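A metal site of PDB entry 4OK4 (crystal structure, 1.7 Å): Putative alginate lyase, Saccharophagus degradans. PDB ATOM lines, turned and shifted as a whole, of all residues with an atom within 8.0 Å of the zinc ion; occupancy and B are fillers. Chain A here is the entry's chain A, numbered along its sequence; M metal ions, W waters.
The backbone carbonyl oxygen of Gln 460 sits at hydrogen-bond distance from a ring nitrogen (ND1) of His 464, at 2.9 Å. ND1 of His 415 lies close to O of Ala 458 (3.2 Å). The side-chain amide oxygen of Asn 310 is in hydrogen-bond range of the backbone NH of His 415. NE2 of His 415 sits at hydrogen-bond distance from OD1 of Asp 311, at 2.8 Å. OD2 of Asp 433 is in hydrogen-bond range of ND2 of Asn 420 (3.3 Å).
Ala 458 touches the zinc ion. Four residues have an atom within 4 Å of the zinc ion: His 415, Asp 433, Ala 458 and His 464.
The zinc ion is bound by water W1 (2.1 Å), NE2 of His 464 (2.1 Å), water W3 (2.2 Å), water W2 (2.2 Å), ND1 of His 415 (2.2 Å) and OD1 of Asp 433 (2.3 Å). The zinc ion has six donor atoms within binding distance.
Water W2 lies within hydrogen-bond range of OD2 of Asp 417 (2.6 Å), OD2 of Asp 433 (2.7 Å) and N of Asn 310 (2.9 Å). Water W3 lies within hydrogen-bond range of the backbone carbonyl oxygen of Ala 458 (2.8 Å) and the backbone carbonyl oxygen of Gly 435 (2.9 Å). Water W1 lies within hydrogen-bond range of the backbone carbonyl oxygen (O) of Asn 310 (2.6 Å), the backbone carbonyl oxygen (O) of Pro 308 (2.7 Å) and the backbone NH (N) of Gly 435 (3.3 Å).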
ATOM      1  N   PRO A 308      24.312  -5.761 -31.925  1.00  0.00           N
ATOM      2  CA  PRO A 308      25.470  -5.299 -31.175  1.00  0.00           C
ATOM      3  C   PRO A 308      25.499  -5.792 -29.727  1.00  0.00           C
ATOM      4  O   PRO A 308      25.625  -4.987 -28.800  1.00  0.00           O
ATOM      5  CB  PRO A 308      25.324  -3.766 -31.225  1.00  0.00           C
ATOM      6  CG  PRO A 308      23.857  -3.553 -31.291  1.00  0.00           C
ATOM      7  CD  PRO A 308      23.299  -4.708 -32.079  1.00  0.00           C
ATOM      8  N   ILE A 309      25.403  -7.109 -29.542  1.00  0.00           N
ATOM      9  CA  ILE A 309      25.484  -7.702 -28.208  1.00  0.00           C
ATOM     10  C   ILE A 309      26.932  -8.056 -27.887  1.00  0.00           C
ATOM     11  O   ILE A 309      27.729  -8.343 -28.793  1.00  0.00           O
ATOM     12  CB  ILE A 309      24.565  -8.931 -28.040  1.00  0.00           C
ATOM     13  CG1 ILE A 309      24.894 -10.019 -29.075  1.00  0.00           C
ATOM     14  CG2 ILE A 309      23.108  -8.512 -28.150  1.00  0.00           C
ATOM     15  CD1 ILE A 309      24.216 -11.344 -28.808  1.00  0.00           C
ATOM     16  N   ASN A 310      27.275  -8.019 -26.603  1.00  0.00           N
ATOM     17  CA  ASN A 310      28.653  -8.150 -26.134  1.00  0.00           C
ATOM     18  C   ASN A 310      29.524  -7.061 -26.754  1.00  0.00           C
ATOM     19  O   ASN A 310      29.004  -6.048 -27.211  1.00  0.00           O
ATOM     20  CB  ASN A 310      29.173  -9.573 -26.415  1.00  0.00           C
ATOM     21  CG  ASN A 310      28.446 -10.626 -25.605  1.00  0.00           C
ATOM     22  OD1 ASN A 310      27.888 -10.330 -24.542  1.00  0.00           O
ATOM     23  ND2 ASN A 310      28.445 -11.857 -26.098  1.00  0.00           N
ATOM     24  N   ASP A 311      30.840  -7.218 -26.734  1.00  0.00           N
ATOM     25  CA  ASP A 311      31.693  -6.207 -27.392  1.00  0.00           C
ATOM     26  C   ASP A 311      31.386  -6.178 -28.881  1.00  0.00           C
ATOM     27  O   ASP A 311      31.440  -7.207 -29.566  1.00  0.00           O
ATOM     28  CB  ASP A 311      33.177  -6.442 -27.122  1.00  0.00           C
ATOM     29  CG  ASP A 311      33.596  -6.049 -25.720  1.00  0.00           C
ATOM     30  OD1 ASP A 311      32.835  -5.353 -25.002  1.00  0.00           O
ATOM     31  OD2 ASP A 311      34.706  -6.438 -25.336  1.00  0.00           O
ATOM     32  N   ALA A 312      31.038  -4.985 -29.383  1.00  0.00           N
ATOM     33  CA  ALA A 312      30.524  -4.835 -30.733  1.00  0.00           C
ATOM     34  C   ALA A 312      30.439  -3.368 -31.123  1.00  0.00           C
ATOM     35  O   ALA A 312      30.175  -2.520 -30.273  1.00  0.00           O
ATOM     36  CB  ALA A 312      29.133  -5.450 -30.852  1.00  0.00           C
ATOM     37  N   LYS A 405      18.653 -12.300 -25.283  1.00  0.00           N
ATOM     38  CA  LYS A 405      20.021 -12.704 -24.993  1.00  0.00           C
ATOM     39  C   LYS A 405      20.086 -13.545 -23.721  1.00  0.00           C
ATOM     40  O   LYS A 405      20.388 -13.050 -22.628  1.00  0.00           O
ATOM     41  CB  LYS A 405      20.940 -11.485 -24.911  1.00  0.00           C
ATOM     42  CG  LYS A 405      22.426 -11.824 -24.949  1.00  0.00           C
ATOM     43  CD  LYS A 405      23.274 -10.572 -24.792  1.00  0.00           C
ATOM     44  CE  LYS A 405      24.763 -10.902 -24.780  1.00  0.00           C
ATOM     45  NZ  LYS A 405      25.207 -11.433 -23.469  1.00  0.00           N
ATOM     46  N   HIS A 413      34.998 -10.753 -23.985  1.00  0.00           N
ATOM     47  CA  HIS A 413      34.198  -9.760 -24.726  1.00  0.00           C
ATOM     48  C   HIS A 413      32.737  -9.739 -24.283  1.00  0.00           C
ATOM     49  O   HIS A 413      31.958  -8.889 -24.709  1.00  0.00           O
ATOM     50  CB  HIS A 413      34.325  -9.972 -26.233  1.00  0.00           C
ATOM     51  CG  HIS A 413      35.651  -9.552 -26.794  1.00  0.00           C
ATOM     52  ND1 HIS A 413      36.462 -10.397 -27.512  1.00  0.00           N
ATOM     53  CD2 HIS A 413      36.298  -8.363 -26.735  1.00  0.00           C
ATOM     54  CE1 HIS A 413      37.556  -9.757 -27.866  1.00  0.00           C
ATOM     55  NE2 HIS A 413      37.483  -8.518 -27.417  1.00  0.00           N
ATOM     56  N   GLY A 414      32.381 -10.681 -23.402  1.00  0.00           N
ATOM     57  CA  GLY A 414      31.017 -10.806 -22.922  1.00  0.00           C
ATOM     58  C   GLY A 414      30.582  -9.665 -22.028  1.00  0.00           C
ATOM     59  O   GLY A 414      31.385  -9.079 -21.295  1.00  0.00           O
ATOM     60  N   HIS A 415      29.295  -9.348 -22.101  1.00  0.00           N
ATOM     61  CA  HIS A 415      28.707  -8.322 -21.245  1.00  0.00           C
ATOM     62  C   HIS A 415      27.923  -8.940 -20.096  1.00  0.00           C
ATOM     63  O   HIS A 415      27.477 -10.085 -20.187  1.00  0.00           O
ATOM     64  CB  HIS A 415      27.858  -7.376 -22.086  1.00  0.00           C
ATOM     65  CG  HIS A 415      28.676  -6.477 -22.952  1.00  0.00           C
ATOM     66  ND1 HIS A 415      28.152  -5.380 -23.603  1.00  0.00           N
ATOM     67  CD2 HIS A 415      29.993  -6.497 -23.262  1.00  0.00           C
ATOM     68  CE1 HIS A 415      29.111  -4.772 -24.270  1.00  0.00           C
ATOM     69  NE2 HIS A 415      30.236  -5.429 -24.084  1.00  0.00           N
ATOM     70  N   PHE A 416      27.784  -8.196 -18.998  1.00  0.00           N
ATOM     71  CA  PHE A 416      27.094  -8.704 -17.817  1.00  0.00           C
ATOM     72  C   PHE A 416      25.599  -8.395 -17.929  1.00  0.00           C
ATOM     73  O   PHE A 416      25.074  -7.550 -17.221  1.00  0.00           O
ATOM     74  CB  PHE A 416      27.737  -8.145 -16.543  1.00  0.00           C
ATOM     75  CG  PHE A 416      29.175  -8.560 -16.375  1.00  0.00           C
ATOM     76  CD1 PHE A 416      29.497  -9.819 -15.862  1.00  0.00           C
ATOM     77  CD2 PHE A 416      30.204  -7.702 -16.745  1.00  0.00           C
ATOM     78  CE1 PHE A 416      30.818 -10.195 -15.709  1.00  0.00           C
ATOM     79  CE2 PHE A 416      31.527  -8.080 -16.602  1.00  0.00           C
ATOM     80  CZ  PHE A 416      31.840  -9.329 -16.093  1.00  0.00           C
ATOM     81  N   ASP A 417      24.940  -9.094 -18.843  1.00  0.00           N
ATOM     82  CA  ASP A 417      23.585  -8.755 -19.241  1.00  0.00           C
ATOM     83  C   ASP A 417      22.694  -9.972 -19.495  1.00  0.00           C
ATOM     84  O   ASP A 417      22.042 -10.071 -20.531  1.00  0.00           O
ATOM     85  CB  ASP A 417      23.619  -7.832 -20.465  1.00  0.00           C
ATOM     86  CG  ASP A 417      24.232  -8.487 -21.699  1.00  0.00           C
ATOM     87  OD1 ASP A 417      24.976  -9.485 -21.555  1.00  0.00           O
ATOM     88  OD2 ASP A 417      23.965  -8.003 -22.808  1.00  0.00           O
ATOM     89  N   ASN A 420      19.009  -9.982 -21.203  1.00  0.00           N
ATOM     90  CA  ASN A 420      18.865  -8.736 -21.945  1.00  0.00           C
ATOM     91  C   ASN A 420      18.010  -8.922 -23.198  1.00  0.00           C
ATOM     92  O   ASN A 420      17.890 -10.035 -23.725  1.00  0.00           O
ATOM     93  CB  ASN A 420      20.241  -8.181 -22.321  1.00  0.00           C
ATOM     94  CG  ASN A 420      20.185  -6.755 -22.842  1.00  0.00           C
ATOM     95  OD1 ASN A 420      19.292  -5.994 -22.469  1.00  0.00           O
ATOM     96  ND2 ASN A 420      21.137  -6.387 -23.685  1.00  0.00           N
ATOM     97  N   LEU A 422      16.819  -6.847 -27.123  1.00  0.00           N
ATOM     98  CA  LEU A 422      16.863  -5.760 -28.092  1.00  0.00           C
ATOM     99  C   LEU A 422      15.584  -5.817 -28.930  1.00  0.00           C
ATOM    100  O   LEU A 422      15.000  -6.880 -29.141  1.00  0.00           O
ATOM    101  CB  LEU A 422      18.081  -5.888 -29.024  1.00  0.00           C
ATOM    102  CG  LEU A 422      19.524  -5.689 -28.515  1.00  0.00           C
ATOM    103  CD1 LEU A 422      19.962  -6.744 -27.503  1.00  0.00           C
ATOM    104  CD2 LEU A 422      20.468  -5.692 -29.710  1.00  0.00           C
ATOM    105  N   THR A 432      17.633  -0.718 -27.359  1.00  0.00           N
ATOM    106  CA  THR A 432      19.005  -0.833 -27.856  1.00  0.00           C
ATOM    107  C   THR A 432      20.019  -1.455 -26.907  1.00  0.00           C
ATOM    108  O   THR A 432      19.831  -1.515 -25.701  1.00  0.00           O
ATOM    109  CB  THR A 432      19.549   0.542 -28.340  1.00  0.00           C
ATOM    110  OG1 THR A 432      19.709   1.415 -27.217  1.00  0.00           O
ATOM    111  CG2 THR A 432      18.595   1.177 -29.345  1.00  0.00           C
ATOM    112  N   ASP A 433      21.121  -1.913 -27.503  1.00  0.00           N
ATOM    113  CA  ASP A 433      22.293  -2.370 -26.775  1.00  0.00           C
ATOM    114  C   ASP A 433      23.415  -1.427 -27.182  1.00  0.00           C
ATOM    115  O   ASP A 433      23.584  -1.145 -28.368  1.00  0.00           O
ATOM    116  CB  ASP A 433      22.605  -3.826 -27.162  1.00  0.00           C
ATOM    117  CG  ASP A 433      23.513  -4.538 -26.157  1.00  0.00           C
ATOM    118  OD1 ASP A 433      24.402  -3.906 -25.556  1.00  0.00           O
ATOM    119  OD2 ASP A 433      23.355  -5.770 -25.990  1.00  0.00           O
ATOM    120  N   TYR A 434      24.161  -0.937 -26.198  1.00  0.00           N
ATOM    121  CA  TYR A 434      25.187   0.085 -26.419  1.00  0.00           C
ATOM    122  C   TYR A 434      26.344  -0.409 -27.309  1.00  0.00           C
ATOM    123  O   TYR A 434      26.959   0.376 -28.034  1.00  0.00           O
ATOM    124  CB  TYR A 434      25.745   0.574 -25.080  1.00  0.00           C
ATOM    125  CG  TYR A 434      26.581   1.826 -25.224  1.00  0.00           C
ATOM    126  CD1 TYR A 434      27.964   1.756 -25.399  1.00  0.00           C
ATOM    127  CD2 TYR A 434      25.974   3.085 -25.230  1.00  0.00           C
ATOM    128  CE1 TYR A 434      28.726   2.909 -25.563  1.00  0.00           C
ATOM    129  CE2 TYR A 434      26.724   4.241 -25.387  1.00  0.00           C
ATOM    130  CZ  TYR A 434      28.105   4.141 -25.555  1.00  0.00           C
ATOM    131  OH  TYR A 434      28.846   5.285 -25.721  1.00  0.00           O
ATOM    132  N   GLY A 435      26.634  -1.695 -27.240  1.00  0.00           N
ATOM    133  CA  GLY A 435      27.828  -2.242 -27.875  1.00  0.00           C
ATOM    134  C   GLY A 435      29.036  -1.870 -27.035  1.00  0.00           C
ATOM    135  O   GLY A 435      28.921  -1.708 -25.815  1.00  0.00           O
ATOM    136  N   ALA A 436      30.177  -1.717 -27.688  1.00  0.00           N
ATOM    137  CA  ALA A 436      31.424  -1.431 -27.000  1.00  0.00           C
ATOM    138  C   ALA A 436      31.766   0.063 -27.001  1.00  0.00           C
ATOM    139  O   ALA A 436      31.326   0.797 -27.880  1.00  0.00           O
ATOM    140  CB  ALA A 436      32.562  -2.220 -27.641  1.00  0.00           C
ATOM    141  N   ASN A 454      34.809   0.989 -21.576  1.00  0.00           N
ATOM    142  CA  ASN A 454      34.253  -0.273 -22.040  1.00  0.00           C
ATOM    143  C   ASN A 454      33.953  -1.200 -20.865  1.00  0.00           C
ATOM    144  O   ASN A 454      32.879  -1.800 -20.807  1.00  0.00           O
ATOM    145  CB  ASN A 454      35.136  -0.975 -23.080  1.00  0.00           C
ATOM    146  CG  ASN A 454      34.403  -2.104 -23.775  1.00  0.00           C
ATOM    147  OD1 ASN A 454      34.740  -3.277 -23.631  1.00  0.00           O
ATOM    148  ND2 ASN A 454      33.356  -1.751 -24.503  1.00  0.00           N
ATOM    149  N   TRP A 457      31.574   1.152 -18.124  1.00  0.00           N
ATOM    150  CA  TRP A 457      30.216   1.414 -18.598  1.00  0.00           C
ATOM    151  C   TRP A 457      29.627   0.272 -19.435  1.00  0.00           C
ATOM    152  O   TRP A 457      28.665  -0.367 -19.021  1.00  0.00           O
ATOM    153  CB  TRP A 457      30.124   2.738 -19.381  1.00  0.00           C
ATOM    154  CG  TRP A 457      28.826   2.859 -20.157  1.00  0.00           C
ATOM    155  CD1 TRP A 457      28.677   2.785 -21.529  1.00  0.00           C
ATOM    156  CD2 TRP A 457      27.501   3.009 -19.619  1.00  0.00           C
ATOM    157  NE1 TRP A 457      27.347   2.898 -21.862  1.00  0.00           N
ATOM    158  CE2 TRP A 457      26.613   3.034 -20.717  1.00  0.00           C
ATOM    159  CE3 TRP A 457      26.996   3.133 -18.324  1.00  0.00           C
ATOM    160  CZ2 TRP A 457      25.225   3.175 -20.548  1.00  0.00           C
ATOM    161  CZ3 TRP A 457      25.617   3.273 -18.153  1.00  0.00           C
ATOM    162  CH2 TRP A 457      24.753   3.302 -19.269  1.00  0.00           C
ATOM    163  N   ALA A 458      30.215   0.023 -20.608  1.00  0.00           N
ATOM    164  CA  ALA A 458      29.569  -0.774 -21.643  1.00  0.00           C
ATOM    165  C   ALA A 458      29.258  -2.220 -21.244  1.00  0.00           C
ATOM    166  O   ALA A 458      28.259  -2.781 -21.701  1.00  0.00           O
ATOM    167  CB  ALA A 458      30.394  -0.750 -22.914  1.00  0.00           C
ATOM    168  N   LYS A 459      30.110  -2.809 -20.410  1.00  0.00           N
ATOM    169  CA  LYS A 459      29.911  -4.201 -19.995  1.00  0.00           C
ATOM    170  C   LYS A 459      28.933  -4.346 -18.834  1.00  0.00           C
ATOM    171  O   LYS A 459      28.407  -5.445 -18.595  1.00  0.00           O
ATOM    172  CB  LYS A 459      31.247  -4.836 -19.597  1.00  0.00           C
ATOM    173  CG  LYS A 459      32.119  -5.246 -20.765  1.00  0.00           C
ATOM    174  CD  LYS A 459      33.339  -6.013 -20.271  1.00  0.00           C
ATOM    175  CE  LYS A 459      34.237  -6.430 -21.413  1.00  0.00           C
ATOM    176  NZ  LYS A 459      35.565  -6.874 -20.892  1.00  0.00           N
ATOM    177  N   GLN A 460      28.687  -3.251 -18.120  1.00  0.00           N
ATOM    178  CA  GLN A 460      27.933  -3.306 -16.863  1.00  0.00           C
ATOM    179  C   GLN A 460      26.443  -3.525 -17.095  1.00  0.00           C
ATOM    180  O   GLN A 460      25.904  -3.130 -18.120  1.00  0.00           O
ATOM    181  CB  GLN A 460      28.188  -2.032 -16.042  1.00  0.00           C
ATOM    182  CG  GLN A 460      29.640  -1.827 -15.647  1.00  0.00           C
ATOM    183  CD  GLN A 460      30.222  -3.009 -14.885  1.00  0.00           C
ATOM    184  OE1 GLN A 460      29.610  -3.501 -13.935  1.00  0.00           O
ATOM    185  NE2 GLN A 460      31.395  -3.478 -15.303  1.00  0.00           N
ATOM    186  N   ALA A 463      23.909  -0.673 -17.912  1.00  0.00           N
ATOM    187  CA  ALA A 463      23.981  -0.220 -19.306  1.00  0.00           C
ATOM    188  C   ALA A 463      23.096  -1.038 -20.258  1.00  0.00           C
ATOM    189  O   ALA A 463      23.035  -0.747 -21.459  1.00  0.00           O
ATOM    190  CB  ALA A 463      25.427  -0.236 -19.783  1.00  0.00           C
ATOM    191  N   HIS A 464      22.396  -2.048 -19.723  1.00  0.00           N
ATOM    192  CA  HIS A 464      21.545  -2.932 -20.531  1.00  0.00           C
ATOM    193  C   HIS A 464      20.080  -2.972 -20.085  1.00  0.00           C
ATOM    194  O   HIS A 464      19.753  -2.489 -18.998  1.00  0.00           O
ATOM    195  CB  HIS A 464      22.111  -4.351 -20.527  1.00  0.00           C
ATOM    196  CG  HIS A 464      23.467  -4.434 -21.168  1.00  0.00           C
ATOM    197  ND1 HIS A 464      24.628  -4.122 -20.498  1.00  0.00           N
ATOM    198  CD2 HIS A 464      23.832  -4.762 -22.429  1.00  0.00           C
ATOM    199  CE1 HIS A 464      25.653  -4.268 -21.309  1.00  0.00           C
ATOM    200  NE2 HIS A 464      25.199  -4.653 -22.490  1.00  0.00           N
ATOM    201  N   ASN A 465      19.239  -3.583 -20.911  1.00  0.00           N
ATOM    202  CA  ASN A 465      17.799  -3.695 -20.652  1.00  0.00           C
ATOM    203  C   ASN A 465      17.445  -4.938 -19.839  1.00  0.00           C
ATOM    204  O   ASN A 465      16.627  -5.766 -20.262  1.00  0.00           O
ATOM    205  CB  ASN A 465      17.016  -3.695 -21.967  1.00  0.00           C
ATOM    206  CG  ASN A 465      17.431  -2.573 -22.890  1.00  0.00           C
ATOM    207  OD1 ASN A 465      17.378  -1.405 -22.526  1.00  0.00           O
ATOM    208  ND2 ASN A 465      17.847  -2.937 -24.104  1.00  0.00           N
HETATM  209 ZN    ZN M   1      26.139  -4.804 -24.357  1.00  0.00          ZN
HETATM  210  O   HOH W   1      26.829  -4.871 -26.331  1.00  0.00           O
HETATM  211  O   HOH W   2      25.427  -6.851 -24.670  1.00  0.00           O
HETATM  212  O   HOH W   3      26.822  -2.770 -24.118  1.00  0.00           O
